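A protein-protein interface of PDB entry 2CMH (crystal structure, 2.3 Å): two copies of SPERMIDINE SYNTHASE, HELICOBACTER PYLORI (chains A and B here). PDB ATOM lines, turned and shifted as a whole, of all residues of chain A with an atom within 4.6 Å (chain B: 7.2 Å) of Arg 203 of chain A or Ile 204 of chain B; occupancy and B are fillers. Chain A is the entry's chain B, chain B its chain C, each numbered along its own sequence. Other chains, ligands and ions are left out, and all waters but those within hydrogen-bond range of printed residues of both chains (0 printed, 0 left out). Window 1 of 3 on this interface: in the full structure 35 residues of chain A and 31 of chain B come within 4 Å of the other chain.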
ATOM      1  N   ILE A  57      -0.090  -1.251  18.381  1.00  0.00           N
ATOM      2  CA  ILE A  57       0.423  -2.600  18.150  1.00  0.00           C
ATOM      3  C   ILE A  57      -0.153  -3.642  19.100  1.00  0.00           C
ATOM      4  O   ILE A  57      -0.836  -4.576  18.669  1.00  0.00           O
ATOM      5  CB  ILE A  57       1.958  -2.647  18.253  1.00  0.00           C
ATOM      6  CG1 ILE A  57       2.588  -1.767  17.161  1.00  0.00           C
ATOM      7  CG2 ILE A  57       2.442  -4.111  18.157  1.00  0.00           C
ATOM      8  CD1 ILE A  57       4.098  -1.646  17.285  1.00  0.00           C
ATOM      9  N   GLU A  58       0.132  -3.485  20.393  1.00  0.00           N
ATOM     10  CA  GLU A  58      -0.361  -4.425  21.396  1.00  0.00           C
ATOM     11  C   GLU A  58      -1.889  -4.404  21.523  1.00  0.00           C
ATOM     12  O   GLU A  58      -2.513  -5.457  21.678  1.00  0.00           O
ATOM     13  CB  GLU A  58       0.271  -4.128  22.757  1.00  0.00           C
ATOM     14  CG  GLU A  58      -0.056  -5.152  23.827  1.00  0.00           C
ATOM     15  CD  GLU A  58       0.501  -4.766  25.179  1.00  0.00           C
ATOM     16  OE1 GLU A  58       0.017  -3.775  25.763  1.00  0.00           O
ATOM     17  OE2 GLU A  58       1.429  -5.444  25.655  1.00  0.00           O
ATOM     18  N   HIS A 173       8.880 -12.978  27.984  1.00  0.00           N
ATOM     19  CA  HIS A 173       9.328 -13.337  26.654  1.00  0.00           C
ATOM     20  C   HIS A 173      10.022 -14.707  26.779  1.00  0.00           C
ATOM     21  O   HIS A 173      10.861 -14.910  27.660  1.00  0.00           O
ATOM     22  CB  HIS A 173      10.301 -12.284  26.126  1.00  0.00           C
ATOM     23  CG  HIS A 173      10.660 -12.460  24.685  1.00  0.00           C
ATOM     24  ND1 HIS A 173      10.030 -11.769  23.671  1.00  0.00           N
ATOM     25  CD2 HIS A 173      11.576 -13.253  24.084  1.00  0.00           C
ATOM     26  CE1 HIS A 173      10.545 -12.130  22.510  1.00  0.00           C
ATOM     27  NE2 HIS A 173      11.486 -13.030  22.731  1.00  0.00           N
ATOM     28  N   ALA A 200       4.559 -10.558  20.067  1.00  0.00           N
ATOM     29  CA  ALA A 200       4.121  -9.520  19.152  1.00  0.00           C
ATOM     30  C   ALA A 200       5.223  -9.284  18.137  1.00  0.00           C
ATOM     31  O   ALA A 200       6.220  -8.616  18.418  1.00  0.00           O
ATOM     32  CB  ALA A 200       3.804  -8.249  19.899  1.00  0.00           C
ATOM     33  N   PRO A 201       5.057  -9.867  16.939  1.00  0.00           N
ATOM     34  CA  PRO A 201       6.012  -9.758  15.834  1.00  0.00           C
ATOM     35  C   PRO A 201       6.445  -8.327  15.513  1.00  0.00           C
ATOM     36  O   PRO A 201       5.627  -7.407  15.493  1.00  0.00           O
ATOM     37  CB  PRO A 201       5.269 -10.414  14.676  1.00  0.00           C
ATOM     38  CG  PRO A 201       4.471 -11.485  15.353  1.00  0.00           C
ATOM     39  CD  PRO A 201       3.930 -10.747  16.565  1.00  0.00           C
ATOM     40  N   LEU A 202       7.743  -8.167  15.257  1.00  0.00           N
ATOM     41  CA  LEU A 202       8.381  -6.888  14.942  1.00  0.00           C
ATOM     42  C   LEU A 202       8.489  -5.930  16.135  1.00  0.00           C
ATOM     43  O   LEU A 202       9.049  -4.829  16.008  1.00  0.00           O
ATOM     44  CB  LEU A 202       7.702  -6.200  13.755  1.00  0.00           C
ATOM     45  CG  LEU A 202       7.958  -6.818  12.376  1.00  0.00           C
ATOM     46  CD1 LEU A 202       9.459  -6.907  12.126  1.00  0.00           C
ATOM     47  CD2 LEU A 202       7.356  -8.193  12.300  1.00  0.00           C
ATOM     48  N   ARG A 203       7.963  -6.349  17.288  1.00  0.00           N
ATOM     49  CA  ARG A 203       8.063  -5.556  18.515  1.00  0.00           C
ATOM     50  C   ARG A 203       9.341  -5.968  19.266  1.00  0.00           C
ATOM     51  O   ARG A 203       9.290  -6.747  20.229  1.00  0.00           O
ATOM     52  CB  ARG A 203       6.832  -5.778  19.407  1.00  0.00           C
ATOM     53  CG  ARG A 203       5.680  -4.820  19.169  1.00  0.00           C
ATOM     54  CD  ARG A 203       5.525  -3.827  20.325  1.00  0.00           C
ATOM     55  NE  ARG A 203       4.905  -4.427  21.509  1.00  0.00           N
ATOM     56  CZ  ARG A 203       4.667  -3.774  22.648  1.00  0.00           C
ATOM     57  NH1 ARG A 203       4.096  -4.403  23.673  1.00  0.00           N
ATOM     58  NH2 ARG A 203       5.006  -2.498  22.773  1.00  0.00           N
ATOM     59  N   ILE A 204      10.487  -5.465  18.813  1.00  0.00           N
ATOM     60  CA  ILE A 204      11.768  -5.790  19.450  1.00  0.00           C
ATOM     61  C   ILE A 204      12.062  -4.998  20.722  1.00  0.00           C
ATOM     62  O   ILE A 204      12.966  -5.349  21.474  1.00  0.00           O
ATOM     63  CB  ILE A 204      12.967  -5.563  18.495  1.00  0.00           C
ATOM     64  CG1 ILE A 204      13.015  -4.098  18.056  1.00  0.00           C
ATOM     65  CG2 ILE A 204      12.885  -6.507  17.311  1.00  0.00           C
ATOM     66  CD1 ILE A 204      14.270  -3.738  17.252  1.00  0.00           C
ATOM     67  N   LEU A 205      11.313  -3.929  20.954  1.00  0.00           N
ATOM     68  CA  LEU A 205      11.521  -3.084  22.129  1.00  0.00           C
ATOM     69  C   LEU A 205      10.827  -3.548  23.406  1.00  0.00           C
ATOM     70  O   LEU A 205      10.742  -2.778  24.356  1.00  0.00           O
ATOM     71  CB  LEU A 205      11.072  -1.650  21.832  1.00  0.00           C
ATOM     72  CG  LEU A 205      11.868  -0.827  20.824  1.00  0.00           C
ATOM     73  CD1 LEU A 205      11.053   0.381  20.363  1.00  0.00           C
ATOM     74  CD2 LEU A 205      13.169  -0.397  21.471  1.00  0.00           C
ATOM     75  N   SER A 206      10.329  -4.782  23.452  1.00  0.00           N
ATOM     76  CA  SER A 206       9.649  -5.257  24.660  1.00  0.00           C
ATOM     77  C   SER A 206       9.951  -6.704  25.064  1.00  0.00           C
ATOM     78  O   SER A 206       9.953  -7.611  24.226  1.00  0.00           O
ATOM     79  CB  SER A 206       8.140  -5.075  24.505  1.00  0.00           C
ATOM     80  OG  SER A 206       7.665  -5.766  23.364  1.00  0.00           O
ATOM     81  N   TYR A 210       2.894 -13.557  25.750  1.00  0.00           N
ATOM     82  CA  TYR A 210       1.476 -13.743  26.017  1.00  0.00           C
ATOM     83  C   TYR A 210       1.017 -15.179  25.809  1.00  0.00           C
ATOM     84  O   TYR A 210       1.668 -15.976  25.122  1.00  0.00           O
ATOM     85  CB  TYR A 210       0.614 -12.846  25.116  1.00  0.00           C
ATOM     86  CG  TYR A 210       1.163 -11.455  24.885  1.00  0.00           C
ATOM     87  CD1 TYR A 210       2.144 -11.220  23.926  1.00  0.00           C
ATOM     88  CD2 TYR A 210       0.705 -10.374  25.637  1.00  0.00           C
ATOM     89  CE1 TYR A 210       2.654  -9.946  23.720  1.00  0.00           C
ATOM     90  CE2 TYR A 210       1.206  -9.098  25.438  1.00  0.00           C
ATOM     91  CZ  TYR A 210       2.171  -8.891  24.483  1.00  0.00           C
ATOM     92  OH  TYR A 210       2.624  -7.612  24.273  1.00  0.00           O
ATOM     93  N   LYS B  13      22.074   0.489  25.068  1.00  0.00           N
ATOM     94  CA  LYS B  13      21.867  -0.700  25.870  1.00  0.00           C
ATOM     95  C   LYS B  13      23.051  -0.795  26.809  1.00  0.00           C
ATOM     96  O   LYS B  13      24.180  -0.510  26.419  1.00  0.00           O
ATOM     97  CB  LYS B  13      21.802  -1.962  25.000  1.00  0.00           C
ATOM     98  CG  LYS B  13      20.531  -2.125  24.186  1.00  0.00           C
ATOM     99  CD  LYS B  13      20.493  -3.500  23.545  1.00  0.00           C
ATOM    100  CE  LYS B  13      19.247  -3.689  22.704  1.00  0.00           C
ATOM    101  NZ  LYS B  13      19.216  -5.028  22.055  1.00  0.00           N
ATOM    102  N   HIS B 173      16.669  -3.151  11.178  1.00  0.00           N
ATOM    103  CA  HIS B 173      15.379  -3.702  11.507  1.00  0.00           C
ATOM    104  C   HIS B 173      14.282  -2.902  10.799  1.00  0.00           C
ATOM    105  O   HIS B 173      14.194  -1.672  10.932  1.00  0.00           O
ATOM    106  CB  HIS B 173      15.168  -3.708  13.010  1.00  0.00           C
ATOM    107  CG  HIS B 173      13.919  -4.403  13.433  1.00  0.00           C
ATOM    108  ND1 HIS B 173      12.718  -3.746  13.600  1.00  0.00           N
ATOM    109  CD2 HIS B 173      13.684  -5.703  13.731  1.00  0.00           C
ATOM    110  CE1 HIS B 173      11.799  -4.613  13.988  1.00  0.00           C
ATOM    111  NE2 HIS B 173      12.360  -5.806  14.075  1.00  0.00           N
ATOM    112  N   LEU B 175      11.192  -2.209  11.309  1.00  0.00           N
ATOM    113  CA  LEU B 175      10.245  -1.351  12.029  1.00  0.00           C
ATOM    114  C   LEU B 175      10.950  -0.156  12.666  1.00  0.00           C
ATOM    115  O   LEU B 175      10.570   1.003  12.465  1.00  0.00           O
ATOM    116  CB  LEU B 175       9.530  -2.149  13.122  1.00  0.00           C
ATOM    117  CG  LEU B 175       8.042  -1.871  13.365  1.00  0.00           C
ATOM    118  CD1 LEU B 175       7.674  -2.386  14.747  1.00  0.00           C
ATOM    119  CD2 LEU B 175       7.712  -0.385  13.259  1.00  0.00           C
ATOM    120  N   ALA B 200      14.702 -12.181  12.443  1.00  0.00           N
ATOM    121  CA  ALA B 200      14.860 -13.413  13.202  1.00  0.00           C
ATOM    122  C   ALA B 200      13.799 -13.436  14.284  1.00  0.00           C
ATOM    123  O   ALA B 200      13.950 -12.808  15.339  1.00  0.00           O
ATOM    124  CB  ALA B 200      16.240 -13.489  13.817  1.00  0.00           C
ATOM    125  N   PRO B 201      12.711 -14.181  14.044  1.00  0.00           N
ATOM    126  CA  PRO B 201      11.637 -14.250  15.035  1.00  0.00           C
ATOM    127  C   PRO B 201      12.169 -14.564  16.435  1.00  0.00           C
ATOM    128  O   PRO B 201      13.021 -15.441  16.621  1.00  0.00           O
ATOM    129  CB  PRO B 201      10.732 -15.356  14.493  1.00  0.00           C
ATOM    130  CG  PRO B 201      11.000 -15.330  13.004  1.00  0.00           C
ATOM    131  CD  PRO B 201      12.490 -15.157  12.962  1.00  0.00           C
ATOM    132  N   LEU B 202      11.662 -13.822  17.412  1.00  0.00           N
ATOM    133  CA  LEU B 202      12.036 -13.988  18.811  1.00  0.00           C
ATOM    134  C   LEU B 202      13.421 -13.440  19.157  1.00  0.00           C
ATOM    135  O   LEU B 202      13.725 -13.239  20.331  1.00  0.00           O
ATOM    136  CB  LEU B 202      11.959 -15.458  19.217  1.00  0.00           C
ATOM    137  CG  LEU B 202      10.617 -16.197  19.184  1.00  0.00           C
ATOM    138  CD1 LEU B 202       9.627 -15.481  20.083  1.00  0.00           C
ATOM    139  CD2 LEU B 202      10.070 -16.281  17.760  1.00  0.00           C
ATOM    140  N   ARG B 203      14.272 -13.210  18.156  1.00  0.00           N
ATOM    141  CA  ARG B 203      15.593 -12.647  18.436  1.00  0.00           C
ATOM    142  C   ARG B 203      15.424 -11.141  18.713  1.00  0.00           C
ATOM    143  O   ARG B 203      15.935 -10.287  17.997  1.00  0.00           O
ATOM    144  CB  ARG B 203      16.552 -12.897  17.262  1.00  0.00           C
ATOM    145  CG  ARG B 203      17.935 -12.296  17.459  1.00  0.00           C
ATOM    146  CD  ARG B 203      19.003 -13.260  17.014  1.00  0.00           C
ATOM    147  NE  ARG B 203      19.896 -12.676  16.027  1.00  0.00           N
ATOM    148  CZ  ARG B 203      21.126 -12.228  16.272  1.00  0.00           C
ATOM    149  NH1 ARG B 203      21.652 -12.297  17.489  1.00  0.00           N
ATOM    150  NH2 ARG B 203      21.829 -11.688  15.282  1.00  0.00           N
ATOM    151  N   ILE B 204      14.684 -10.854  19.782  1.00  0.00           N
ATOM    152  CA  ILE B 204      14.363  -9.499  20.207  1.00  0.00           C
ATOM    153  C   ILE B 204      15.574  -8.660  20.644  1.00  0.00           C
ATOM    154  O   ILE B 204      15.421  -7.505  21.055  1.00  0.00           O
ATOM    155  CB  ILE B 204      13.283  -9.563  21.354  1.00  0.00           C
ATOM    156  CG1 ILE B 204      12.032  -8.782  20.966  1.00  0.00           C
ATOM    157  CG2 ILE B 204      13.830  -9.094  22.678  1.00  0.00           C
ATOM    158  CD1 ILE B 204      11.146  -9.509  19.984  1.00  0.00           C
ATOM    159  N   LEU B 205      16.780  -9.208  20.498  1.00  0.00           N
ATOM    160  CA  LEU B 205      17.990  -8.508  20.947  1.00  0.00           C
ATOM    161  C   LEU B 205      18.802  -7.613  20.016  1.00  0.00           C
ATOM    162  O   LEU B 205      19.755  -6.974  20.462  1.00  0.00           O
ATOM    163  CB  LEU B 205      18.944  -9.508  21.611  1.00  0.00           C
ATOM    164  CG  LEU B 205      19.138  -9.286  23.113  1.00  0.00           C
ATOM    165  CD1 LEU B 205      19.958  -8.013  23.335  1.00  0.00           C
ATOM    166  CD2 LEU B 205      17.775  -9.186  23.819  1.00  0.00           C
ATOM    167  N   SER B 206      18.454  -7.529  18.743  1.00  0.00           N
ATOM    168  CA  SER B 206      19.249  -6.670  17.879  1.00  0.00           C
ATOM    169  C   SER B 206      18.454  -5.826  16.899  1.00  0.00           C
ATOM    170  O   SER B 206      17.368  -6.208  16.469  1.00  0.00           O
ATOM    171  CB  SER B 206      20.296  -7.529  17.145  1.00  0.00           C
ATOM    172  OG  SER B 206      19.700  -8.701  16.615  1.00  0.00           O
ATOM    173  N   ASN B 207      18.995  -4.655  16.579  1.00  0.00           N
ATOM    174  CA  ASN B 207      18.372  -3.770  15.604  1.00  0.00           C
ATOM    175  C   ASN B 207      18.923  -4.289  14.283  1.00  0.00           C
ATOM    176  O   ASN B 207      19.789  -3.667  13.664  1.00  0.00           O
ATOM    177  CB  ASN B 207      18.825  -2.338  15.828  1.00  0.00           C
ATOM    178  CG  ASN B 207      18.305  -1.377  14.772  1.00  0.00           C
ATOM    179  OD1 ASN B 207      18.524  -0.173  14.885  1.00  0.00           O
ATOM    180  ND2 ASN B 207      17.624  -1.892  13.753  1.00  0.00           N
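The side-chain carboxylate (OE2) of Glu 58 of chain A lies within salt-bridge range of the guanidinium group (NH1) of Arg 203 of chain A (3.5 Å).
A ring nitrogen (ND1) of His 173 of chain B sits at hydrogen-bond distance from the backbone NH (N) of Leu 175 of chain B, 3.2 Å away.
ND2 of Asn 207 of chain B lies close to N of His 173 of chain B (3.0 Å).
Arg 203 of chain A touches just one residue of chain B: Ile 204 (3.3 Å).
Of the printed residues of chain A, Ile 204 of chain B touches His 173 (3.7 Å), Arg 203 (3.3 Å) and Ile 204 (3.3 Å).
Of the printed residues of chain B, Ile 204 of chain A touches His 173 (3.4 Å) and Ile 204 (3.3 Å).
Of the printed residues of chain B, His 173 of chain A touches Leu 202 and Ile 204.
The nearest printed residue of chain B that does not touch Leu 202 of chain A is Ile 204 of chain B (5.9 Å).
A ring nitrogen (NE2) of His 173 of chain A lies within hydrogen-bond range of the backbone carbonyl oxygen (O) of Leu 202 of chain B (3.3 Å).
The backbone carbonyl oxygen (O) of Ile 204 of chain B lies close to the backbone carbonyl oxygen (O) of Ile 204 of chain A (3.3 Å).
Of the 11 printed residues of chain B, 4 touch a printed residue of chain A.
Hydrophobic or aromatic side chains of chain A that line the printed part of chain B: His 173, Leu 202 and Ile 204.
Along chain A the printed residues that touch a printed residue of chain B span positions 173 to 204.
Among the printed residues, 7 pairs touch across the chains.
Among the printed residues, no Asp or Glu carboxylate lies within 4 Å of a Lys or Arg side-chain nitrogen of the other chain.
His 173 of chain A touches Leu 202 of chain B, and with the chains exchanged Leu 202 of chain A touches His 173 of chain B.
His 173 of chain A touches Ile 204 of chain B, and with the chains exchanged Ile 204 of chain A touches His 173 of chain B.
Arg 203 of chain A touches Ile 204 of chain B, but with the chains exchanged Ile 204 of chain A does not touch Arg 203 of chain B (4.9 Å).
Ile 204 of chain A touches its own counterpart, Ile 204 of chain B.
8 positions are printed for both chains.
Of the 7 pairs that touch across the chains among the printed residues, 5 have their exchanged pair printed and touching as well.
Ile 204 of chain B touches His 173 of chain A (CD1 to CE1, 3.7 Å).
Leu 202 of chain A touches His 173 of chain B (O to CE1, 3.4 Å).
Leu 175 of chain B touches Leu 202 of chain A.
Arg 203 of chain A touches Ile 204 of chain B (O to CD1, 3.3 Å).
His 173 of chain B touches Ile 204 of chain A (NE2 to CG2, 3.4 Å).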
